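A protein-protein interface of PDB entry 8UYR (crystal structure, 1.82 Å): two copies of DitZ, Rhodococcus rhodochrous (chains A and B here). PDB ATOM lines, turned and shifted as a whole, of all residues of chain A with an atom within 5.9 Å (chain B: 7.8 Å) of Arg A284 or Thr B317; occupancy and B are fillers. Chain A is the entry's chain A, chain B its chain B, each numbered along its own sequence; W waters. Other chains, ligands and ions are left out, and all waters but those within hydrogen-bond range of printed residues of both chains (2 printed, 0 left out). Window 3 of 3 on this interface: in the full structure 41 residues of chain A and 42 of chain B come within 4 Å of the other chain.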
ATOM      1  N   LEU A 279     -11.639  -1.839 -11.447  1.00  0.00           N
ATOM      2  CA  LEU A 279     -11.711  -3.292 -11.297  1.00  0.00           C
ATOM      3  C   LEU A 279     -12.156  -3.957 -12.595  1.00  0.00           C
ATOM      4  O   LEU A 279     -11.675  -5.044 -12.933  1.00  0.00           O
ATOM      5  CB  LEU A 279     -12.650  -3.657 -10.149  1.00  0.00           C
ATOM      6  CG  LEU A 279     -12.166  -3.341  -8.722  1.00  0.00           C
ATOM      7  CD1 LEU A 279     -13.203  -3.789  -7.721  1.00  0.00           C
ATOM      8  CD2 LEU A 279     -10.833  -4.010  -8.433  1.00  0.00           C
ATOM      9  N   ASP A 280     -13.077  -3.332 -13.337  1.00  0.00           N
ATOM     10  CA  ASP A 280     -13.488  -3.898 -14.619  1.00  0.00           C
ATOM     11  C   ASP A 280     -12.288  -4.046 -15.541  1.00  0.00           C
ATOM     12  O   ASP A 280     -12.095  -5.090 -16.166  1.00  0.00           O
ATOM     13  CB  ASP A 280     -14.554  -3.023 -15.294  1.00  0.00           C
ATOM     14  CG  ASP A 280     -15.956  -3.215 -14.705  1.00  0.00           C
ATOM     15  OD1 ASP A 280     -16.130  -4.035 -13.774  1.00  0.00           O
ATOM     16  OD2 ASP A 280     -16.886  -2.526 -15.174  1.00  0.00           O
ATOM     17  N   ARG A 281     -11.457  -3.008 -15.621  1.00  0.00           N
ATOM     18  CA  ARG A 281     -10.299  -3.075 -16.498  1.00  0.00           C
ATOM     19  C   ARG A 281      -9.266  -4.064 -15.979  1.00  0.00           C
ATOM     20  O   ARG A 281      -8.688  -4.826 -16.759  1.00  0.00           O
ATOM     21  CB  ARG A 281      -9.677  -1.693 -16.668  1.00  0.00           C
ATOM     22  CG  ARG A 281      -8.564  -1.712 -17.683  1.00  0.00           C
ATOM     23  CD  ARG A 281      -8.092  -0.329 -18.114  1.00  0.00           C
ATOM     24  NE  ARG A 281      -7.110  -0.485 -19.186  1.00  0.00           N
ATOM     25  CZ  ARG A 281      -7.429  -0.738 -20.456  1.00  0.00           C
ATOM     26  NH1 ARG A 281      -8.707  -0.836 -20.816  1.00  0.00           N
ATOM     27  NH2 ARG A 281      -6.475  -0.884 -21.369  1.00  0.00           N
ATOM     28  N   LEU A 282      -9.006  -4.065 -14.670  1.00  0.00           N
ATOM     29  CA  LEU A 282      -8.038  -5.019 -14.129  1.00  0.00           C
ATOM     30  C   LEU A 282      -8.528  -6.452 -14.302  1.00  0.00           C
ATOM     31  O   LEU A 282      -7.771  -7.329 -14.740  1.00  0.00           O
ATOM     32  CB  LEU A 282      -7.770  -4.725 -12.656  1.00  0.00           C
ATOM     33  CG  LEU A 282      -6.765  -3.671 -12.226  1.00  0.00           C
ATOM     34  CD1 LEU A 282      -6.937  -3.422 -10.752  1.00  0.00           C
ATOM     35  CD2 LEU A 282      -5.359  -4.119 -12.503  1.00  0.00           C
ATOM     36  N   ASP A 283      -9.784  -6.717 -13.920  1.00  0.00           N
ATOM     37  CA  ASP A 283     -10.347  -8.057 -14.061  1.00  0.00           C
ATOM     38  C   ASP A 283     -10.165  -8.564 -15.483  1.00  0.00           C
ATOM     39  O   ASP A 283      -9.704  -9.690 -15.696  1.00  0.00           O
ATOM     40  CB  ASP A 283     -11.837  -8.070 -13.689  1.00  0.00           C
ATOM     41  CG  ASP A 283     -12.093  -8.181 -12.184  1.00  0.00           C
ATOM     42  OD1 ASP A 283     -11.157  -8.436 -11.402  1.00  0.00           O
ATOM     43  OD2 ASP A 283     -13.267  -8.018 -11.775  1.00  0.00           O
ATOM     44  N   ARG A 284     -10.511  -7.731 -16.473  1.00  0.00           N
ATOM     45  CA  ARG A 284     -10.398  -8.149 -17.866  1.00  0.00           C
ATOM     46  C   ARG A 284      -8.941  -8.354 -18.266  1.00  0.00           C
ATOM     47  O   ARG A 284      -8.627  -9.275 -19.031  1.00  0.00           O
ATOM     48  CB  ARG A 284     -11.070  -7.115 -18.769  1.00  0.00           C
ATOM     49  CG  ARG A 284     -10.839  -7.316 -20.258  1.00  0.00           C
ATOM     50  CD  ARG A 284     -11.680  -6.327 -21.069  1.00  0.00           C
ATOM     51  NE  ARG A 284     -11.880  -5.075 -20.346  1.00  0.00           N
ATOM     52  CZ  ARG A 284     -11.393  -3.895 -20.717  1.00  0.00           C
ATOM     53  NH1 ARG A 284     -10.675  -3.772 -21.827  1.00  0.00           N
ATOM     54  NH2 ARG A 284     -11.636  -2.827 -19.976  1.00  0.00           N
ATOM     55  N   HIS A 285      -8.036  -7.510 -17.760  1.00  0.00           N
ATOM     56  CA  HIS A 285      -6.617  -7.697 -18.053  1.00  0.00           C
ATOM     57  C   HIS A 285      -6.112  -9.055 -17.562  1.00  0.00           C
ATOM     58  O   HIS A 285      -5.369  -9.745 -18.271  1.00  0.00           O
ATOM     59  CB  HIS A 285      -5.796  -6.579 -17.423  1.00  0.00           C
ATOM     60  CG  HIS A 285      -4.353  -6.621 -17.807  1.00  0.00           C
ATOM     61  ND1 HIS A 285      -3.350  -6.939 -16.915  1.00  0.00           N
ATOM     62  CD2 HIS A 285      -3.750  -6.438 -19.004  1.00  0.00           C
ATOM     63  CE1 HIS A 285      -2.188  -6.921 -17.542  1.00  0.00           C
ATOM     64  NE2 HIS A 285      -2.403  -6.617 -18.809  1.00  0.00           N
ATOM     65  N   ILE A 286      -6.489  -9.448 -16.346  1.00  0.00           N
ATOM     66  CA  ILE A 286      -6.007 -10.719 -15.811  1.00  0.00           C
ATOM     67  C   ILE A 286      -6.545 -11.891 -16.625  1.00  0.00           C
ATOM     68  O   ILE A 286      -5.829 -12.868 -16.879  1.00  0.00           O
ATOM     69  CB  ILE A 286      -6.367 -10.838 -14.321  1.00  0.00           C
ATOM     70  CG1 ILE A 286      -5.427  -9.970 -13.492  1.00  0.00           C
ATOM     71  CG2 ILE A 286      -6.284 -12.289 -13.853  1.00  0.00           C
ATOM     72  CD1 ILE A 286      -3.974 -10.426 -13.537  1.00  0.00           C
ATOM     73  N   VAL A 287      -7.808 -11.819 -17.051  1.00  0.00           N
ATOM     74  CA  VAL A 287      -8.355 -12.863 -17.915  1.00  0.00           C
ATOM     75  C   VAL A 287      -7.587 -12.918 -19.230  1.00  0.00           C
ATOM     76  O   VAL A 287      -7.133 -13.983 -19.663  1.00  0.00           O
ATOM     77  CB  VAL A 287      -9.857 -12.625 -18.152  1.00  0.00           C
ATOM     78  CG1 VAL A 287     -10.347 -13.460 -19.326  1.00  0.00           C
ATOM     79  CG2 VAL A 287     -10.649 -12.943 -16.893  1.00  0.00           C
ATOM     80  N   ASN A 288      -7.406 -11.763 -19.870  1.00  0.00           N
ATOM     81  CA  ASN A 288      -6.781 -11.719 -21.188  1.00  0.00           C
ATOM     82  C   ASN A 288      -5.294 -12.048 -21.159  1.00  0.00           C
ATOM     83  O   ASN A 288      -4.730 -12.405 -22.199  1.00  0.00           O
ATOM     84  CB  ASN A 288      -6.974 -10.335 -21.808  1.00  0.00           C
ATOM     85  CG  ASN A 288      -8.403 -10.075 -22.207  1.00  0.00           C
ATOM     86  OD1 ASN A 288      -9.167 -11.005 -22.460  1.00  0.00           O
ATOM     87  ND2 ASN A 288      -8.775  -8.803 -22.276  1.00  0.00           N
ATOM     88  N   GLN A 289      -4.636 -11.901 -20.015  1.00  0.00           N
ATOM     89  CA  GLN A 289      -3.213 -12.184 -19.913  1.00  0.00           C
ATOM     90  C   GLN A 289      -2.930 -13.490 -19.181  1.00  0.00           C
ATOM     91  O   GLN A 289      -1.768 -13.781 -18.899  1.00  0.00           O
ATOM     92  CB  GLN A 289      -2.494 -11.024 -19.229  1.00  0.00           C
ATOM     93  CG  GLN A 289      -2.465  -9.745 -20.071  1.00  0.00           C
ATOM     94  CD  GLN A 289      -1.577  -9.872 -21.297  1.00  0.00           C
ATOM     95  OE1 GLN A 289      -2.057 -10.082 -22.414  1.00  0.00           O
ATOM     96  NE2 GLN A 289      -0.270  -9.740 -21.092  1.00  0.00           N
ATOM     97  N   LYS B  69      -2.086 -13.368 -29.039  1.00  0.00           N
ATOM     98  CA  LYS B  69      -1.803 -12.390 -27.991  1.00  0.00           C
ATOM     99  C   LYS B  69      -0.310 -12.256 -27.717  1.00  0.00           C
ATOM    100  O   LYS B  69       0.177 -11.151 -27.438  1.00  0.00           O
ATOM    101  CB  LYS B  69      -2.552 -12.771 -26.720  1.00  0.00           C
ATOM    102  CG  LYS B  69      -4.028 -12.458 -26.792  1.00  0.00           C
ATOM    103  CD  LYS B  69      -4.695 -12.770 -25.470  1.00  0.00           C
ATOM    104  CE  LYS B  69      -5.813 -11.790 -25.198  1.00  0.00           C
ATOM    105  NZ  LYS B  69      -6.877 -11.918 -26.236  1.00  0.00           N
ATOM    106  N   MET B 238      -2.873   0.131 -17.918  1.00  0.00           N
ATOM    107  CA  MET B 238      -4.002   0.152 -16.999  1.00  0.00           C
ATOM    108  C   MET B 238      -4.504   1.568 -16.758  1.00  0.00           C
ATOM    109  O   MET B 238      -5.716   1.784 -16.667  1.00  0.00           O
ATOM    110  CB  MET B 238      -3.631  -0.512 -15.668  1.00  0.00           C
ATOM    111  CG  MET B 238      -3.582  -2.039 -15.726  1.00  0.00           C
ATOM    112  SD  MET B 238      -5.222  -2.698 -16.079  1.00  0.00           S
ATOM    113  CE  MET B 238      -6.200  -1.579 -15.065  1.00  0.00           C
ATOM    114  N   PRO B 241      -6.568   4.623 -20.074  1.00  0.00           N
ATOM    115  CA  PRO B 241      -7.979   4.911 -20.360  1.00  0.00           C
ATOM    116  C   PRO B 241      -8.827   5.312 -19.165  1.00  0.00           C
ATOM    117  O   PRO B 241     -10.033   5.513 -19.345  1.00  0.00           O
ATOM    118  CB  PRO B 241      -8.470   3.578 -20.926  1.00  0.00           C
ATOM    119  CG  PRO B 241      -7.726   2.590 -20.150  1.00  0.00           C
ATOM    120  CD  PRO B 241      -6.347   3.172 -19.931  1.00  0.00           C
ATOM    121  N   LEU B 242      -8.265   5.451 -17.965  1.00  0.00           N
ATOM    122  CA  LEU B 242      -9.086   5.630 -16.773  1.00  0.00           C
ATOM    123  C   LEU B 242      -9.008   7.042 -16.188  1.00  0.00           C
ATOM    124  O   LEU B 242      -9.568   7.282 -15.114  1.00  0.00           O
ATOM    125  CB  LEU B 242      -8.704   4.592 -15.710  1.00  0.00           C
ATOM    126  CG  LEU B 242      -8.775   3.090 -16.043  1.00  0.00           C
ATOM    127  CD1 LEU B 242      -8.214   2.262 -14.883  1.00  0.00           C
ATOM    128  CD2 LEU B 242     -10.185   2.638 -16.370  1.00  0.00           C
ATOM    129  N   GLY B 271     -14.262   5.462 -21.381  1.00  0.00           N
ATOM    130  CA  GLY B 271     -15.041   4.650 -20.462  1.00  0.00           C
ATOM    131  C   GLY B 271     -16.213   5.421 -19.878  1.00  0.00           C
ATOM    132  O   GLY B 271     -16.487   6.560 -20.267  1.00  0.00           O
ATOM    133  N   VAL B 272     -16.911   4.799 -18.917  1.00  0.00           N
ATOM    134  CA  VAL B 272     -18.119   5.382 -18.336  1.00  0.00           C
ATOM    135  C   VAL B 272     -17.970   5.682 -16.848  1.00  0.00           C
ATOM    136  O   VAL B 272     -18.455   6.718 -16.370  1.00  0.00           O
ATOM    137  CB  VAL B 272     -19.351   4.486 -18.576  1.00  0.00           C
ATOM    138  CG1 VAL B 272     -20.621   5.195 -18.086  1.00  0.00           C
ATOM    139  CG2 VAL B 272     -19.473   4.123 -20.042  1.00  0.00           C
ATOM    140  N   CYS B 314     -17.976   7.407 -23.850  1.00  0.00           N
ATOM    141  CA  CYS B 314     -17.703   6.454 -24.920  1.00  0.00           C
ATOM    142  C   CYS B 314     -16.951   5.259 -24.348  1.00  0.00           C
ATOM    143  O   CYS B 314     -15.925   5.446 -23.696  1.00  0.00           O
ATOM    144  CB  CYS B 314     -16.870   7.120 -26.035  1.00  0.00           C
ATOM    145  SG  CYS B 314     -17.544   8.744 -26.607  1.00  0.00           S
ATOM    146  N   TYR B 315     -17.425   4.038 -24.616  1.00  0.00           N
ATOM    147  CA  TYR B 315     -16.780   2.869 -24.023  1.00  0.00           C
ATOM    148  C   TYR B 315     -16.898   1.638 -24.904  1.00  0.00           C
ATOM    149  O   TYR B 315     -17.854   1.492 -25.669  1.00  0.00           O
ATOM    150  CB  TYR B 315     -17.358   2.546 -22.641  1.00  0.00           C
ATOM    151  CG  TYR B 315     -18.636   1.717 -22.618  1.00  0.00           C
ATOM    152  CD1 TYR B 315     -19.862   2.279 -22.956  1.00  0.00           C
ATOM    153  CD2 TYR B 315     -18.623   0.388 -22.195  1.00  0.00           C
ATOM    154  CE1 TYR B 315     -21.031   1.540 -22.897  1.00  0.00           C
ATOM    155  CE2 TYR B 315     -19.795  -0.360 -22.131  1.00  0.00           C
ATOM    156  CZ  TYR B 315     -20.992   0.219 -22.484  1.00  0.00           C
ATOM    157  OH  TYR B 315     -22.162  -0.504 -22.418  1.00  0.00           O
ATOM    158  N   ILE B 316     -15.911   0.738 -24.761  1.00  0.00           N
ATOM    159  CA  ILE B 316     -15.849  -0.523 -25.494  1.00  0.00           C
ATOM    160  C   ILE B 316     -16.528  -1.614 -24.679  1.00  0.00           C
ATOM    161  O   ILE B 316     -17.508  -2.231 -25.113  1.00  0.00           O
ATOM    162  CB  ILE B 316     -14.401  -0.945 -25.789  1.00  0.00           C
ATOM    163  CG1 ILE B 316     -13.587   0.173 -26.421  1.00  0.00           C
ATOM    164  CG2 ILE B 316     -14.372  -2.221 -26.680  1.00  0.00           C
ATOM    165  CD1 ILE B 316     -12.107  -0.066 -26.230  1.00  0.00           C
ATOM    166  N   THR B 317     -15.981  -1.877 -23.498  1.00  0.00           N
ATOM    167  CA  THR B 317     -16.526  -2.864 -22.584  1.00  0.00           C
ATOM    168  C   THR B 317     -16.302  -2.351 -21.172  1.00  0.00           C
ATOM    169  O   THR B 317     -15.225  -1.837 -20.856  1.00  0.00           O
ATOM    170  CB  THR B 317     -15.878  -4.249 -22.780  1.00  0.00           C
ATOM    171  OG1 THR B 317     -16.313  -5.128 -21.732  1.00  0.00           O
ATOM    172  CG2 THR B 317     -14.367  -4.159 -22.737  1.00  0.00           C
ATOM    173  N   GLU B 318     -17.328  -2.449 -20.346  1.00  0.00           N
ATOM    174  CA  GLU B 318     -17.260  -2.002 -18.965  1.00  0.00           C
ATOM    175  C   GLU B 318     -18.488  -2.554 -18.252  1.00  0.00           C
ATOM    176  O   GLU B 318     -19.499  -1.855 -18.119  1.00  0.00           O
ATOM    177  CB  GLU B 318     -17.199  -0.470 -18.887  1.00  0.00           C
ATOM    178  CG  GLU B 318     -16.750   0.047 -17.526  1.00  0.00           C
ATOM    179  CD  GLU B 318     -16.705   1.552 -17.452  1.00  0.00           C
ATOM    180  OE1 GLU B 318     -16.225   2.169 -18.423  1.00  0.00           O
ATOM    181  OE2 GLU B 318     -17.144   2.115 -16.419  1.00  0.00           O
ATOM    182  N   PRO B 319     -18.451  -3.822 -17.837  1.00  0.00           N
ATOM    183  CA  PRO B 319     -19.665  -4.471 -17.311  1.00  0.00           C
ATOM    184  C   PRO B 319     -20.366  -3.706 -16.207  1.00  0.00           C
ATOM    185  O   PRO B 319     -21.591  -3.825 -16.071  1.00  0.00           O
ATOM    186  CB  PRO B 319     -19.133  -5.814 -16.792  1.00  0.00           C
ATOM    187  CG  PRO B 319     -17.957  -6.108 -17.649  1.00  0.00           C
ATOM    188  CD  PRO B 319     -17.311  -4.755 -17.907  1.00  0.00           C
ATOM    189  N   SER B 320     -19.645  -2.934 -15.402  1.00  0.00           N
ATOM    190  CA  SER B 320     -20.283  -2.223 -14.302  1.00  0.00           C
ATOM    191  C   SER B 320     -20.658  -0.797 -14.662  1.00  0.00           C
ATOM    192  O   SER B 320     -21.290  -0.115 -13.850  1.00  0.00           O
ATOM    193  CB  SER B 320     -19.373  -2.215 -13.071  1.00  0.00           C
ATOM    194  OG  SER B 320     -18.241  -1.397 -13.279  1.00  0.00           O
ATOM    195  N   GLY B 321     -20.292  -0.338 -15.861  1.00  0.00           N
ATOM    196  CA  GLY B 321     -20.462   1.068 -16.192  1.00  0.00           C
ATOM    197  C   GLY B 321     -21.913   1.504 -16.250  1.00  0.00           C
ATOM    198  O   GLY B 321     -22.228   2.656 -15.950  1.00  0.00           O
ATOM    199  N   TRP B 335     -21.415   3.356 -27.417  1.00  0.00           N
ATOM    200  CA  TRP B 335     -20.507   2.226 -27.569  1.00  0.00           C
ATOM    201  C   TRP B 335     -19.458   2.523 -28.635  1.00  0.00           C
ATOM    202  O   TRP B 335     -19.672   3.337 -29.536  1.00  0.00           O
ATOM    203  CB  TRP B 335     -21.262   0.950 -27.952  1.00  0.00           C
ATOM    204  CG  TRP B 335     -20.332  -0.210 -28.168  1.00  0.00           C
ATOM    205  CD1 TRP B 335     -19.662  -0.906 -27.214  1.00  0.00           C
ATOM    206  CD2 TRP B 335     -19.965  -0.788 -29.429  1.00  0.00           C
ATOM    207  NE1 TRP B 335     -18.893  -1.896 -27.799  1.00  0.00           N
ATOM    208  CE2 TRP B 335     -19.064  -1.842 -29.157  1.00  0.00           C
ATOM    209  CE3 TRP B 335     -20.308  -0.515 -30.764  1.00  0.00           C
ATOM    210  CZ2 TRP B 335     -18.505  -2.627 -30.170  1.00  0.00           C
ATOM    211  CZ3 TRP B 335     -19.741  -1.292 -31.772  1.00  0.00           C
ATOM    212  CH2 TRP B 335     -18.854  -2.343 -31.463  1.00  0.00           C
ATOM    213  N   GLU B 336     -18.319   1.834 -28.529  1.00  0.00           N
ATOM    214  CA  GLU B 336     -17.278   1.946 -29.540  1.00  0.00           C
ATOM    215  C   GLU B 336     -16.542   0.624 -29.632  1.00  0.00           C
ATOM    216  O   GLU B 336     -16.448  -0.110 -28.654  1.00  0.00           O
ATOM    217  CB  GLU B 336     -16.297   3.067 -29.216  1.00  0.00           C
ATOM    218  CG  GLU B 336     -15.787   3.023 -27.785  1.00  0.00           C
ATOM    219  CD  GLU B 336     -14.568   3.892 -27.602  1.00  0.00           C
ATOM    220  OE1 GLU B 336     -14.743   5.092 -27.284  1.00  0.00           O
ATOM    221  OE2 GLU B 336     -13.444   3.387 -27.830  1.00  0.00           O
ATOM    222  N   CYS B 337     -16.015   0.333 -30.823  1.00  0.00           N
ATOM    223  CA  CYS B 337     -15.297  -0.916 -31.063  1.00  0.00           C
ATOM    224  C   CYS B 337     -13.791  -0.779 -30.849  1.00  0.00           C
ATOM    225  O   CYS B 337     -13.143  -1.718 -30.369  1.00  0.00           O
ATOM    226  CB  CYS B 337     -15.592  -1.406 -32.484  1.00  0.00           C
ATOM    227  SG  CYS B 337     -14.839  -2.996 -32.879  1.00  0.00           S
ATOM    228  N   SER B 342      -5.597  -3.163 -29.305  1.00  0.00           N
ATOM    229  CA  SER B 342      -5.626  -4.270 -28.355  1.00  0.00           C
ATOM    230  C   SER B 342      -6.897  -4.297 -27.511  1.00  0.00           C
ATOM    231  O   SER B 342      -7.356  -5.373 -27.123  1.00  0.00           O
ATOM    232  CB  SER B 342      -4.399  -4.191 -27.447  1.00  0.00           C
ATOM    233  OG  SER B 342      -4.394  -2.961 -26.749  1.00  0.00           O
ATOM    234  N   ASP B 343      -7.472  -3.133 -27.197  1.00  0.00           N
ATOM    235  CA  ASP B 343      -8.684  -3.095 -26.389  1.00  0.00           C
ATOM    236  C   ASP B 343      -9.943  -3.460 -27.162  1.00  0.00           C
ATOM    237  O   ASP B 343     -11.001  -3.618 -26.548  1.00  0.00           O
ATOM    238  CB  ASP B 343      -8.857  -1.698 -25.766  1.00  0.00           C
ATOM    239  CG  ASP B 343      -7.860  -1.451 -24.654  1.00  0.00           C
ATOM    240  OD1 ASP B 343      -7.931  -2.163 -23.627  1.00  0.00           O
ATOM    241  OD2 ASP B 343      -6.970  -0.593 -24.830  1.00  0.00           O
ATOM    242  N   SER B 344      -9.873  -3.592 -28.479  1.00  0.00           N
ATOM    243  CA  SER B 344     -11.086  -3.857 -29.242  1.00  0.00           C
ATOM    244  C   SER B 344     -11.672  -5.222 -28.884  1.00  0.00           C
ATOM    245  O   SER B 344     -10.954  -6.153 -28.516  1.00  0.00           O
ATOM    246  CB  SER B 344     -10.794  -3.796 -30.743  1.00  0.00           C
ATOM    247  OG  SER B 344     -11.955  -4.125 -31.491  1.00  0.00           O
ATOM    248  N   THR B 345     -12.999  -5.325 -28.978  1.00  0.00           N
ATOM    249  CA  THR B 345     -13.703  -6.590 -28.818  1.00  0.00           C
ATOM    250  C   THR B 345     -13.994  -7.289 -30.147  1.00  0.00           C
ATOM    251  O   THR B 345     -14.672  -8.321 -30.146  1.00  0.00           O
ATOM    252  CB  THR B 345     -15.012  -6.380 -28.047  1.00  0.00           C
ATOM    253  OG1 THR B 345     -15.722  -5.266 -28.599  1.00  0.00           O
ATOM    254  CG2 THR B 345     -14.713  -6.092 -26.587  1.00  0.00           C
ATOM    255  N   THR B 352     -20.103  -9.781 -26.886  1.00  0.00           N
ATOM    256  CA  THR B 352     -19.516  -9.269 -25.657  1.00  0.00           C
ATOM    257  C   THR B 352     -20.353  -8.136 -25.067  1.00  0.00           C
ATOM    258  O   THR B 352     -20.603  -8.108 -23.854  1.00  0.00           O
ATOM    259  CB  THR B 352     -18.086  -8.817 -25.937  1.00  0.00           C
ATOM    260  OG1 THR B 352     -17.328  -9.951 -26.396  1.00  0.00           O
ATOM    261  CG2 THR B 352     -17.449  -8.250 -24.692  1.00  0.00           C
ATOM    262  N   LEU B 353     -20.804  -7.202 -25.904  1.00  0.00           N
ATOM    263  CA  LEU B 353     -21.604  -6.092 -25.391  1.00  0.00           C
ATOM    264  C   LEU B 353     -22.979  -6.569 -24.926  1.00  0.00           C
ATOM    265  O   LEU B 353     -23.449  -6.161 -23.854  1.00  0.00           O
ATOM    266  CB  LEU B 353     -21.740  -5.003 -26.454  1.00  0.00           C
ATOM    267  CG  LEU B 353     -22.483  -3.764 -25.941  1.00  0.00           C
ATOM    268  CD1 LEU B 353     -21.720  -3.121 -24.791  1.00  0.00           C
ATOM    269  CD2 LEU B 353     -22.771  -2.742 -27.048  1.00  0.00           C
ATOM    270  N   GLU B 356     -23.123  -7.808 -21.457  1.00  0.00           N
ATOM    271  CA  GLU B 356     -23.100  -6.725 -20.478  1.00  0.00           C
ATOM    272  C   GLU B 356     -24.441  -6.015 -20.420  1.00  0.00           C
ATOM    273  O   GLU B 356     -24.920  -5.656 -19.336  1.00  0.00           O
ATOM    274  CB  GLU B 356     -22.005  -5.712 -20.816  1.00  0.00           C
ATOM    275  CG  GLU B 356     -20.634  -6.279 -20.839  1.00  0.00           C
ATOM    276  CD  GLU B 356     -19.598  -5.282 -21.313  1.00  0.00           C
ATOM    277  OE1 GLU B 356     -19.754  -4.063 -21.053  1.00  0.00           O
ATOM    278  OE2 GLU B 356     -18.615  -5.726 -21.946  1.00  0.00           O
HETATM  279  O   HOH W   1      -4.496  -0.703 -23.618  1.00  0.00           O
HETATM  280  O   HOH W   2     -13.571  -1.986 -18.603  1.00  0.00           O
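No position is printed for both chains.
OD2 of Asp A280 is in hydrogen-bond range of OG of Ser B320 (2.6 Å). NH2 of Arg A281 lies within salt-bridge range of OD1 of Asp B343, at 3.0 Å. OD1 of Asp B343 is in salt-bridge range of NH1 of Arg A284 (3.7 Å). OD2 of Asp A280 sits close to N of Pro B319, 3.3 Å away.
The backbone carbonyl oxygen of Arg A284 lies close to the side-chain amide nitrogen of Asn A288 (3.3 Å). OE1 of Glu B318 lies within hydrogen-bond range of N of Val B272. The backbone NH (N) of Glu B318 sits at hydrogen-bond distance from the side-chain carboxylate (OE1) of Glu B356 (3.0 Å).
Hydrophobic or aromatic side chains of chain A that line the printed part of chain B: Leu A282. Of the 24 printed residues of chain B, 8 touch a printed residue of chain A. Among the printed residues, 10 pairs touch across the chains. Among the printed residues, Asp or Glu carboxylates within 4 Å of a Lys or Arg side-chain nitrogen of the other chain: Arg A281 with Asp B343 (3.0 Å) and Arg A284 with Asp B343 (3.7 Å).
Water W2 bridges NH2 of Arg A284 (2.5 Å) and O of Thr B317 (2.8 Å). Water W1 bridges OD2 of Asp B343 (2.8 Å) and NH2 of Arg A281 (3.0 Å).
Of the printed residues of chain B, Arg A284 touches Thr B317 and Asp B343. Printed residues of chain A within 4 Å of Thr B317: Arg A284. Printed residues of chain A within 4 Å of Glu B318: Asp A280. Printed residues of chain A within 4 Å of Lys B69: Asn A288 (3.2 Å). Of the printed residues of chain A, Asp B343 touches Arg A281 and Arg A284. The nearest printed residue of chain A that does not touch Thr B317 is Asp A280 (5.7 Å). The nearest printed residue of chain B that does not touch Asn A288 is Ser B342 (6.1 Å).
Among the printed residues, pairs that only touch across the chains: Asp A280 with Glu B318 (3.5 Å), Arg A281 with Met B238 (3.5 Å), Arg A281 with Pro B241 (3.3 Å), Leu A282 with Met B238 (3.6 Å), Arg A284 with Thr B317 (3.6 Å) and Asn A288 with Lys B69 (3.2 Å).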
